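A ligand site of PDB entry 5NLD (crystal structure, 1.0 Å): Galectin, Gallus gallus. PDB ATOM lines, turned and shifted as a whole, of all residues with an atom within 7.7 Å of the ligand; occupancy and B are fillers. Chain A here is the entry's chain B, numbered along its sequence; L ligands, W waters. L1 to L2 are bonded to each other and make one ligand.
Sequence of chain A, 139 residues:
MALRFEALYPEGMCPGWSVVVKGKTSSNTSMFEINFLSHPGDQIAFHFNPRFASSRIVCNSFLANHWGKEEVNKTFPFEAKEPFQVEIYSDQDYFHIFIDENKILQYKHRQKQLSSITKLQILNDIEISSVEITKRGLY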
ATOM      1  N   MET A  31      17.289 -10.632  10.472  1.00  0.00           N
ATOM      2  CA  MET A  31      17.897 -11.520   9.493  1.00  0.00           C
ATOM      3  C   MET A  31      17.213 -11.271   8.167  1.00  0.00           C
ATOM      4  O   MET A  31      16.119 -10.704   8.109  1.00  0.00           O
ATOM      5  CB  MET A  31      17.703 -12.986   9.896  1.00  0.00           C
ATOM      6  CG  MET A  31      16.247 -13.399  10.002  1.00  0.00           C
ATOM      7  SD  MET A  31      16.077 -15.154  10.321  1.00  0.00           S
ATOM      8  CE  MET A  31      16.690 -15.293  11.988  1.00  0.00           C
ATOM      9  N   PHE A  32      17.879 -11.699   7.097  1.00  0.00           N
ATOM     10  CA  PHE A  32      17.244 -11.710   5.778  1.00  0.00           C
ATOM     11  C   PHE A  32      17.650 -12.980   5.074  1.00  0.00           C
ATOM     12  O   PHE A  32      18.538 -13.702   5.524  1.00  0.00           O
ATOM     13  CB  PHE A  32      17.582 -10.449   4.944  1.00  0.00           C
ATOM     14  CG  PHE A  32      18.993 -10.387   4.413  1.00  0.00           C
ATOM     15  CD1 PHE A  32      19.994  -9.795   5.147  1.00  0.00           C
ATOM     16  CD2 PHE A  32      19.303 -10.865   3.148  1.00  0.00           C
ATOM     17  CE1 PHE A  32      21.292  -9.719   4.645  1.00  0.00           C
ATOM     18  CE2 PHE A  32      20.591 -10.781   2.639  1.00  0.00           C
ATOM     19  CZ  PHE A  32      21.586 -10.208   3.388  1.00  0.00           C
ATOM     20  N   GLU A  33      16.991 -13.267   3.950  1.00  0.00           N
ATOM     21  CA  GLU A  33      17.386 -14.431   3.189  1.00  0.00           C
ATOM     22  C   GLU A  33      17.187 -14.197   1.710  1.00  0.00           C
ATOM     23  O   GLU A  33      16.337 -13.403   1.277  1.00  0.00           O
ATOM     24  CB  GLU A  33      16.661 -15.683   3.642  1.00  0.00           C
ATOM     25  CG  GLU A  33      15.195 -15.630   3.455  1.00  0.00           C
ATOM     26  CD  GLU A  33      14.511 -16.743   4.223  1.00  0.00           C
ATOM     27  OE1 GLU A  33      14.018 -17.706   3.593  1.00  0.00           O
ATOM     28  OE2 GLU A  33      14.521 -16.668   5.466  1.00  0.00           O
ATOM     29  N   ASN A  35      16.703 -16.715  -1.588  1.00  0.00           N
ATOM     30  CA  ASN A  35      16.375 -18.068  -1.985  1.00  0.00           C
ATOM     31  C   ASN A  35      16.305 -18.216  -3.494  1.00  0.00           C
ATOM     32  O   ASN A  35      15.779 -17.335  -4.181  1.00  0.00           O
ATOM     33  CB  ASN A  35      15.016 -18.459  -1.406  1.00  0.00           C
ATOM     34  CG  ASN A  35      15.000 -18.436   0.099  1.00  0.00           C
ATOM     35  OD1 ASN A  35      15.962 -18.846   0.751  1.00  0.00           O
ATOM     36  ND2 ASN A  35      13.903 -17.963   0.677  1.00  0.00           N
ATOM     37  N   ILE A  44      13.308 -25.113  -2.628  1.00  0.00           N
ATOM     38  CA  ILE A  44      14.384 -24.140  -2.465  1.00  0.00           C
ATOM     39  C   ILE A  44      15.721 -24.832  -2.717  1.00  0.00           C
ATOM     40  O   ILE A  44      16.239 -25.582  -1.871  1.00  0.00           O
ATOM     41  CB  ILE A  44      14.370 -23.410  -1.111  1.00  0.00           C
ATOM     42  CG1 ILE A  44      12.997 -22.766  -0.842  1.00  0.00           C
ATOM     43  CG2 ILE A  44      15.489 -22.370  -1.083  1.00  0.00           C
ATOM     44  CD1 ILE A  44      12.844 -22.205   0.558  1.00  0.00           C
ATOM     45  N   HIS A  47      19.227 -21.621  -0.153  1.00  0.00           N
ATOM     46  CA  HIS A  47      18.772 -20.659   0.838  1.00  0.00           C
ATOM     47  C   HIS A  47      20.007 -20.097   1.500  1.00  0.00           C
ATOM     48  O   HIS A  47      20.829 -20.855   2.029  1.00  0.00           O
ATOM     49  CB  HIS A  47      17.900 -21.418   1.840  1.00  0.00           C
ATOM     50  CG  HIS A  47      17.593 -20.699   3.126  1.00  0.00           C
ATOM     51  ND1 HIS A  47      16.627 -19.733   3.233  1.00  0.00           N
ATOM     52  CD2 HIS A  47      18.033 -20.933   4.381  1.00  0.00           C
ATOM     53  CE1 HIS A  47      16.522 -19.374   4.505  1.00  0.00           C
ATOM     54  NE2 HIS A  47      17.373 -20.088   5.227  1.00  0.00           N
ATOM     55  N   PHE A  48      20.139 -18.762   1.466  1.00  0.00           N
ATOM     56  CA  PHE A  48      21.274 -18.020   1.997  1.00  0.00           C
ATOM     57  C   PHE A  48      20.718 -17.073   3.053  1.00  0.00           C
ATOM     58  O   PHE A  48      19.951 -16.181   2.705  1.00  0.00           O
ATOM     59  CB  PHE A  48      21.929 -17.243   0.852  1.00  0.00           C
ATOM     60  CG  PHE A  48      22.972 -16.248   1.285  1.00  0.00           C
ATOM     61  CD1 PHE A  48      24.261 -16.638   1.576  1.00  0.00           C
ATOM     62  CD2 PHE A  48      22.655 -14.900   1.396  1.00  0.00           C
ATOM     63  CE1 PHE A  48      25.218 -15.715   1.951  1.00  0.00           C
ATOM     64  CE2 PHE A  48      23.607 -13.960   1.785  1.00  0.00           C
ATOM     65  CZ  PHE A  48      24.893 -14.372   2.065  1.00  0.00           C
ATOM     66  N   ASN A  49      21.098 -17.248   4.321  1.00  0.00           N
ATOM     67  CA  ASN A  49      20.383 -16.587   5.428  1.00  0.00           C
ATOM     68  C   ASN A  49      21.334 -16.003   6.464  1.00  0.00           C
ATOM     69  O   ASN A  49      21.693 -16.670   7.446  1.00  0.00           O
ATOM     70  CB  ASN A  49      19.469 -17.650   6.074  1.00  0.00           C
ATOM     71  CG  ASN A  49      18.674 -17.187   7.297  1.00  0.00           C
ATOM     72  OD1 ASN A  49      18.305 -18.034   8.110  1.00  0.00           O
ATOM     73  ND2 ASN A  49      18.340 -15.916   7.402  1.00  0.00           N
ATOM     74  N   ARG A  51      22.092 -14.224   9.692  1.00  0.00           N
ATOM     75  CA  ARG A  51      21.381 -14.083  10.956  1.00  0.00           C
ATOM     76  C   ARG A  51      22.186 -13.128  11.848  1.00  0.00           C
ATOM     77  O   ARG A  51      23.231 -13.493  12.389  1.00  0.00           O
ATOM     78  CB  ARG A  51      21.184 -15.448  11.617  1.00  0.00           C
ATOM     79  CG  ARG A  51      20.308 -16.398  10.774  1.00  0.00           C
ATOM     80  CD  ARG A  51      19.995 -17.716  11.501  1.00  0.00           C
ATOM     81  NE  ARG A  51      19.175 -18.619  10.676  1.00  0.00           N
ATOM     82  CZ  ARG A  51      18.771 -19.843  11.046  1.00  0.00           C
ATOM     83  NH1 ARG A  51      19.086 -20.322  12.244  1.00  0.00           N
ATOM     84  NH2 ARG A  51      18.061 -20.597  10.225  1.00  0.00           N
ATOM     85  N   VAL A  58      23.563 -18.947   7.570  1.00  0.00           N
ATOM     86  CA  VAL A  58      23.033 -20.317   7.477  1.00  0.00           C
ATOM     87  C   VAL A  58      22.633 -20.543   6.043  1.00  0.00           C
ATOM     88  O   VAL A  58      21.876 -19.751   5.479  1.00  0.00           O
ATOM     89  CB  VAL A  58      21.836 -20.533   8.421  1.00  0.00           C
ATOM     90  CG1 VAL A  58      21.244 -21.932   8.246  1.00  0.00           C
ATOM     91  CG2 VAL A  58      22.268 -20.292   9.861  1.00  0.00           C
ATOM     92  N   CYS A  59      23.126 -21.628   5.448  1.00  0.00           N
ATOM     93  CA  CYS A  59      22.728 -22.037   4.106  1.00  0.00           C
ATOM     94  C   CYS A  59      22.131 -23.445   4.163  1.00  0.00           C
ATOM     95  O   CYS A  59      22.547 -24.286   4.946  1.00  0.00           O
ATOM     96  CB  CYS A  59      23.912 -22.030   3.137  1.00  0.00           C
ATOM     97  SG  CYS A  59      24.563 -20.373   2.801  1.00  0.00           S
ATOM     98  N   ASN A  60      21.152 -23.689   3.296  1.00  0.00           N
ATOM     99  CA  ASN A  60      20.495 -24.981   3.265  1.00  0.00           C
ATOM    100  C   ASN A  60      19.679 -25.079   1.961  1.00  0.00           C
ATOM    101  O   ASN A  60      19.668 -24.153   1.132  1.00  0.00           O
ATOM    102  CB  ASN A  60      19.586 -25.132   4.498  1.00  0.00           C
ATOM    103  CG  ASN A  60      19.401 -26.580   4.966  1.00  0.00           C
ATOM    104  OD1 ASN A  60      19.508 -27.539   4.201  1.00  0.00           O
ATOM    105  ND2 ASN A  60      19.099 -26.728   6.255  1.00  0.00           N
ATOM    106  N   SER A  61      19.002 -26.210   1.801  1.00  0.00           N
ATOM    107  CA  SER A  61      18.075 -26.455   0.700  1.00  0.00           C
ATOM    108  C   SER A  61      16.807 -27.056   1.276  1.00  0.00           C
ATOM    109  O   SER A  61      16.860 -27.820   2.250  1.00  0.00           O
ATOM    110  CB  SER A  61      18.655 -27.435  -0.326  1.00  0.00           C
ATOM    111  OG  SER A  61      19.914 -27.002  -0.837  1.00  0.00           O
ATOM    112  N   PHE A  62      15.671 -26.721   0.647  1.00  0.00           N
ATOM    113  CA  PHE A  62      14.346 -27.213   1.054  1.00  0.00           C
ATOM    114  C   PHE A  62      13.825 -28.085  -0.071  1.00  0.00           C
ATOM    115  O   PHE A  62      13.277 -27.600  -1.049  1.00  0.00           O
ATOM    116  CB  PHE A  62      13.405 -26.034   1.339  1.00  0.00           C
ATOM    117  CG  PHE A  62      12.093 -26.403   1.961  1.00  0.00           C
ATOM    118  CD1 PHE A  62      12.006 -26.675   3.321  1.00  0.00           C
ATOM    119  CD2 PHE A  62      10.939 -26.467   1.199  1.00  0.00           C
ATOM    120  CE1 PHE A  62      10.786 -27.003   3.894  1.00  0.00           C
ATOM    121  CE2 PHE A  62       9.719 -26.796   1.772  1.00  0.00           C
ATOM    122  CZ  PHE A  62       9.647 -27.057   3.124  1.00  0.00           C
ATOM    123  N   TRP A  67      13.896 -29.132   5.161  1.00  0.00           N
ATOM    124  CA  TRP A  67      15.272 -28.704   5.100  1.00  0.00           C
ATOM    125  C   TRP A  67      16.206 -29.903   5.182  1.00  0.00           C
ATOM    126  O   TRP A  67      15.844 -30.956   5.708  1.00  0.00           O
ATOM    127  CB  TRP A  67      15.550 -27.731   6.248  1.00  0.00           C
ATOM    128  CG  TRP A  67      14.788 -26.452   6.120  1.00  0.00           C
ATOM    129  CD1 TRP A  67      13.725 -26.030   6.871  1.00  0.00           C
ATOM    130  CD2 TRP A  67      15.027 -25.412   5.159  1.00  0.00           C
ATOM    131  NE1 TRP A  67      13.294 -24.794   6.434  1.00  0.00           N
ATOM    132  CE2 TRP A  67      14.080 -24.396   5.394  1.00  0.00           C
ATOM    133  CE3 TRP A  67      15.972 -25.244   4.146  1.00  0.00           C
ATOM    134  CZ2 TRP A  67      14.051 -23.220   4.632  1.00  0.00           C
ATOM    135  CZ3 TRP A  67      15.940 -24.074   3.396  1.00  0.00           C
ATOM    136  CH2 TRP A  67      14.979 -23.091   3.638  1.00  0.00           C
ATOM    137  N   GLY A  68      17.422 -29.722   4.661  1.00  0.00           N
ATOM    138  CA  GLY A  68      18.475 -30.695   4.814  1.00  0.00           C
ATOM    139  C   GLY A  68      19.432 -30.259   5.920  1.00  0.00           C
ATOM    140  O   GLY A  68      19.026 -29.560   6.859  1.00  0.00           O
ATOM    141  N   LYS A  69      20.686 -30.660   5.795  1.00  0.00           N
ATOM    142  CA  LYS A  69      21.712 -30.301   6.779  1.00  0.00           C
ATOM    143  C   LYS A  69      22.082 -28.841   6.633  1.00  0.00           C
ATOM    144  O   LYS A  69      22.358 -28.381   5.532  1.00  0.00           O
ATOM    145  CB  LYS A  69      22.953 -31.178   6.583  1.00  0.00           C
ATOM    146  CG  LYS A  69      24.091 -30.911   7.558  1.00  0.00           C
ATOM    147  CD  LYS A  69      25.276 -31.847   7.275  1.00  0.00           C
ATOM    148  CE  LYS A  69      26.406 -31.677   8.285  1.00  0.00           C
ATOM    149  NZ  LYS A  69      25.995 -32.085   9.655  1.00  0.00           N
ATOM    150  N   GLU A  70      22.097 -28.108   7.742  1.00  0.00           N
ATOM    151  CA  GLU A  70      22.550 -26.723   7.707  1.00  0.00           C
ATOM    152  C   GLU A  70      24.054 -26.644   7.480  1.00  0.00           C
ATOM    153  O   GLU A  70      24.820 -27.406   8.074  1.00  0.00           O
ATOM    154  CB  GLU A  70      22.206 -25.980   9.003  1.00  0.00           C
ATOM    155  CG  GLU A  70      20.736 -25.718   9.137  1.00  0.00           C
ATOM    156  CD  GLU A  70      20.351 -24.961  10.398  1.00  0.00           C
ATOM    157  OE1 GLU A  70      21.181 -24.824  11.320  1.00  0.00           O
ATOM    158  OE2 GLU A  70      19.172 -24.532  10.449  1.00  0.00           O
ATOM    159  N   GLU A  71      24.463 -25.715   6.625  1.00  0.00           N
ATOM    160  CA  GLU A  71      25.855 -25.319   6.474  1.00  0.00           C
ATOM    161  C   GLU A  71      25.985 -23.939   7.083  1.00  0.00           C
ATOM    162  O   GLU A  71      25.386 -22.982   6.588  1.00  0.00           O
ATOM    163  CB  GLU A  71      26.267 -25.343   4.991  1.00  0.00           C
ATOM    164  CG  GLU A  71      26.105 -26.742   4.421  1.00  0.00           C
ATOM    165  CD  GLU A  71      26.627 -26.931   3.008  1.00  0.00           C
ATOM    166  OE1 GLU A  71      27.518 -26.190   2.554  1.00  0.00           O
ATOM    167  OE2 GLU A  71      26.151 -27.886   2.346  1.00  0.00           O
ATOM    168  N   VAL A  72      26.736 -23.851   8.171  1.00  0.00           N
ATOM    169  CA  VAL A  72      26.815 -22.627   8.960  1.00  0.00           C
ATOM    170  C   VAL A  72      28.187 -22.019   8.773  1.00  0.00           C
ATOM    171  O   VAL A  72      29.201 -22.698   8.938  1.00  0.00           O
ATOM    172  CB  VAL A  72      26.562 -22.909  10.444  1.00  0.00           C
ATOM    173  CG1 VAL A  72      26.644 -21.633  11.258  1.00  0.00           C
ATOM    174  CG2 VAL A  72      25.194 -23.576  10.638  1.00  0.00           C
ATOM    175  N   LEU A 123      13.733 -12.102   1.214  1.00  0.00           N
ATOM    176  CA  LEU A 123      12.770 -11.953   2.308  1.00  0.00           C
ATOM    177  C   LEU A 123      13.391 -11.299   3.539  1.00  0.00           C
ATOM    178  O   LEU A 123      14.595 -11.418   3.797  1.00  0.00           O
ATOM    179  CB  LEU A 123      12.242 -13.316   2.762  1.00  0.00           C
ATOM    180  CG  LEU A 123      11.832 -14.380   1.751  1.00  0.00           C
ATOM    181  CD1 LEU A 123      11.537 -15.712   2.444  1.00  0.00           C
ATOM    182  CD2 LEU A 123      10.620 -13.925   1.032  1.00  0.00           C
ATOM    183  N   ASN A 124      12.513 -10.671   4.312  1.00  0.00           N
ATOM    184  CA  ASN A 124      12.789 -10.190   5.667  1.00  0.00           C
ATOM    185  C   ASN A 124      13.624  -8.924   5.702  1.00  0.00           C
ATOM    186  O   ASN A 124      13.335  -8.009   4.932  1.00  0.00           O
ATOM    187  CB  ASN A 124      13.216 -11.353   6.554  1.00  0.00           C
ATOM    188  CG  ASN A 124      12.089 -12.362   6.703  1.00  0.00           C
ATOM    189  OD1 ASN A 124      10.911 -11.991   6.681  1.00  0.00           O
ATOM    190  ND2 ASN A 124      12.440 -13.638   6.782  1.00  0.00           N
HETATM  191  C1  LIG L   1      15.914 -25.412  14.363  1.00  0.00           C
HETATM  192  C2  LIG L   1      17.094 -24.739  13.713  1.00  0.00           C
HETATM  193  C3  LIG L   1      16.700 -23.562  12.910  1.00  0.00           C
HETATM  194  C4  LIG L   1      15.608 -23.898  11.930  1.00  0.00           C
HETATM  195  C5  LIG L   1      14.422 -24.490  12.678  1.00  0.00           C
HETATM  196  C6  LIG L   1      13.282 -24.897  11.767  1.00  0.00           C
HETATM  197  O1  LIG L   1      15.406 -24.701  15.428  1.00  0.00           O
HETATM  198  O2  LIG L   1      18.031 -24.357  14.735  1.00  0.00           O
HETATM  199  O3  LIG L   1      17.860 -23.004  12.221  1.00  0.00           O
HETATM  200  O4  LIG L   1      15.182 -22.689  11.261  1.00  0.00           O
HETATM  201  O5  LIG L   1      14.838 -25.663  13.400  1.00  0.00           O
HETATM  202  O6  LIG L   1      13.738 -25.827  10.822  1.00  0.00           O
HETATM  203  C1  LG2 L   2      15.027 -22.813   9.902  1.00  0.00           C
HETATM  204  C2  LG2 L   2      14.378 -21.541   9.370  1.00  0.00           C
HETATM  205  C3  LG2 L   2      14.398 -21.483   7.877  1.00  0.00           C
HETATM  206  C4  LG2 L   2      15.764 -21.697   7.324  1.00  0.00           C
HETATM  207  C5  LG2 L   2      16.428 -22.915   7.931  1.00  0.00           C
HETATM  208  C6  LG2 L   2      17.708 -23.411   7.320  1.00  0.00           C
HETATM  209  O1  LG2 L   2      13.026 -21.481   9.874  1.00  0.00           O
HETATM  210  O2  LG2 L   2      13.884 -20.190   7.455  1.00  0.00           O
HETATM  211  O3  LG2 L   2      16.599 -20.622   7.692  1.00  0.00           O
HETATM  212  O4  LG2 L   2      16.356 -22.982   9.337  1.00  0.00           O
HETATM  213  O5  LG2 L   2      18.139 -24.622   7.895  1.00  0.00           O
HETATM  214  O   HOH W   1      12.313 -21.092  12.692  1.00  0.00           O
HETATM  215  O   HOH W   2      20.583 -23.888  13.837  1.00  0.00           O
HETATM  216  O   HOH W   3      11.493 -19.323   8.863  1.00  0.00           O
HETATM  217  O   HOH W   4      13.034 -19.848   4.912  1.00  0.00           O
HETATM  218  O   HOH W   5      15.322 -17.942   8.129  1.00  0.00           O
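A ring nitrogen (NE2) of His 47 lies within hydrogen-bond range of an oxygen (O3) of LG2 L2 (2.6 Å). OE2 of Glu 70 sits at hydrogen-bond distance from O3 of LIG L1 (2.7 Å). O5 of LG2 L2 lies within hydrogen-bond range of ND2 of Asn 60, at 2.8 Å. An oxygen (O3) of LG2 L2 lies within hydrogen-bond range of the guanidinium group (NH2) of Arg 51. The side-chain amide oxygen (OD1) of Asn 49 is in hydrogen-bond range of an oxygen (O3) of LG2 L2.
A ring nitrogen (ND1) of His 47 sits close to the side-chain carboxylate (OE1) of Glu 33 (3.3 Å). ND1 of His 47 is in hydrogen-bond range of OD1 of Asn 35 (2.7 Å). The backbone carbonyl oxygen of Gly 68 is in hydrogen-bond range of the side-chain amide nitrogen of Asn 60 (2.9 Å). OD1 of Asn 60 lies close to O of Lys 69 (3.3 Å). The guanidinium group (NE) of Arg 51 lies within hydrogen-bond range of the side-chain amide oxygen (OD1) of Asn 49, 2.8 Å away. N of Asn 49 is in hydrogen-bond range of O of Val 58 (2.9 Å). SD of Met 31 sits at hydrogen-bond distance from ND2 of Asn 49 (3.8 Å). O of Phe 32 is in hydrogen-bond range of ND2 of Asn 49 (2.9 Å).
CG1 of Val 58 touches C6 of LG2 L2 (3.9 Å). Trp 67 touches the ligand. Hydrophobic or aromatic side chains within 4 Å of the ligand: His 47, Val 58 and Trp 67. Of the 22 residues printed, 7 come within 4 Å of the ligand. The nearest printed residue that does not touch the ligand is Glu 33 (4.1 Å).
Water W4 bridges OE1 of Glu 33 (2.7 Å) and O2 of LG2 L2 (2.7 Å). Water W2 lies within hydrogen-bond range of O2 of LIG L1 (2.7 Å) and OE1 of Glu 70 (2.8 Å).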
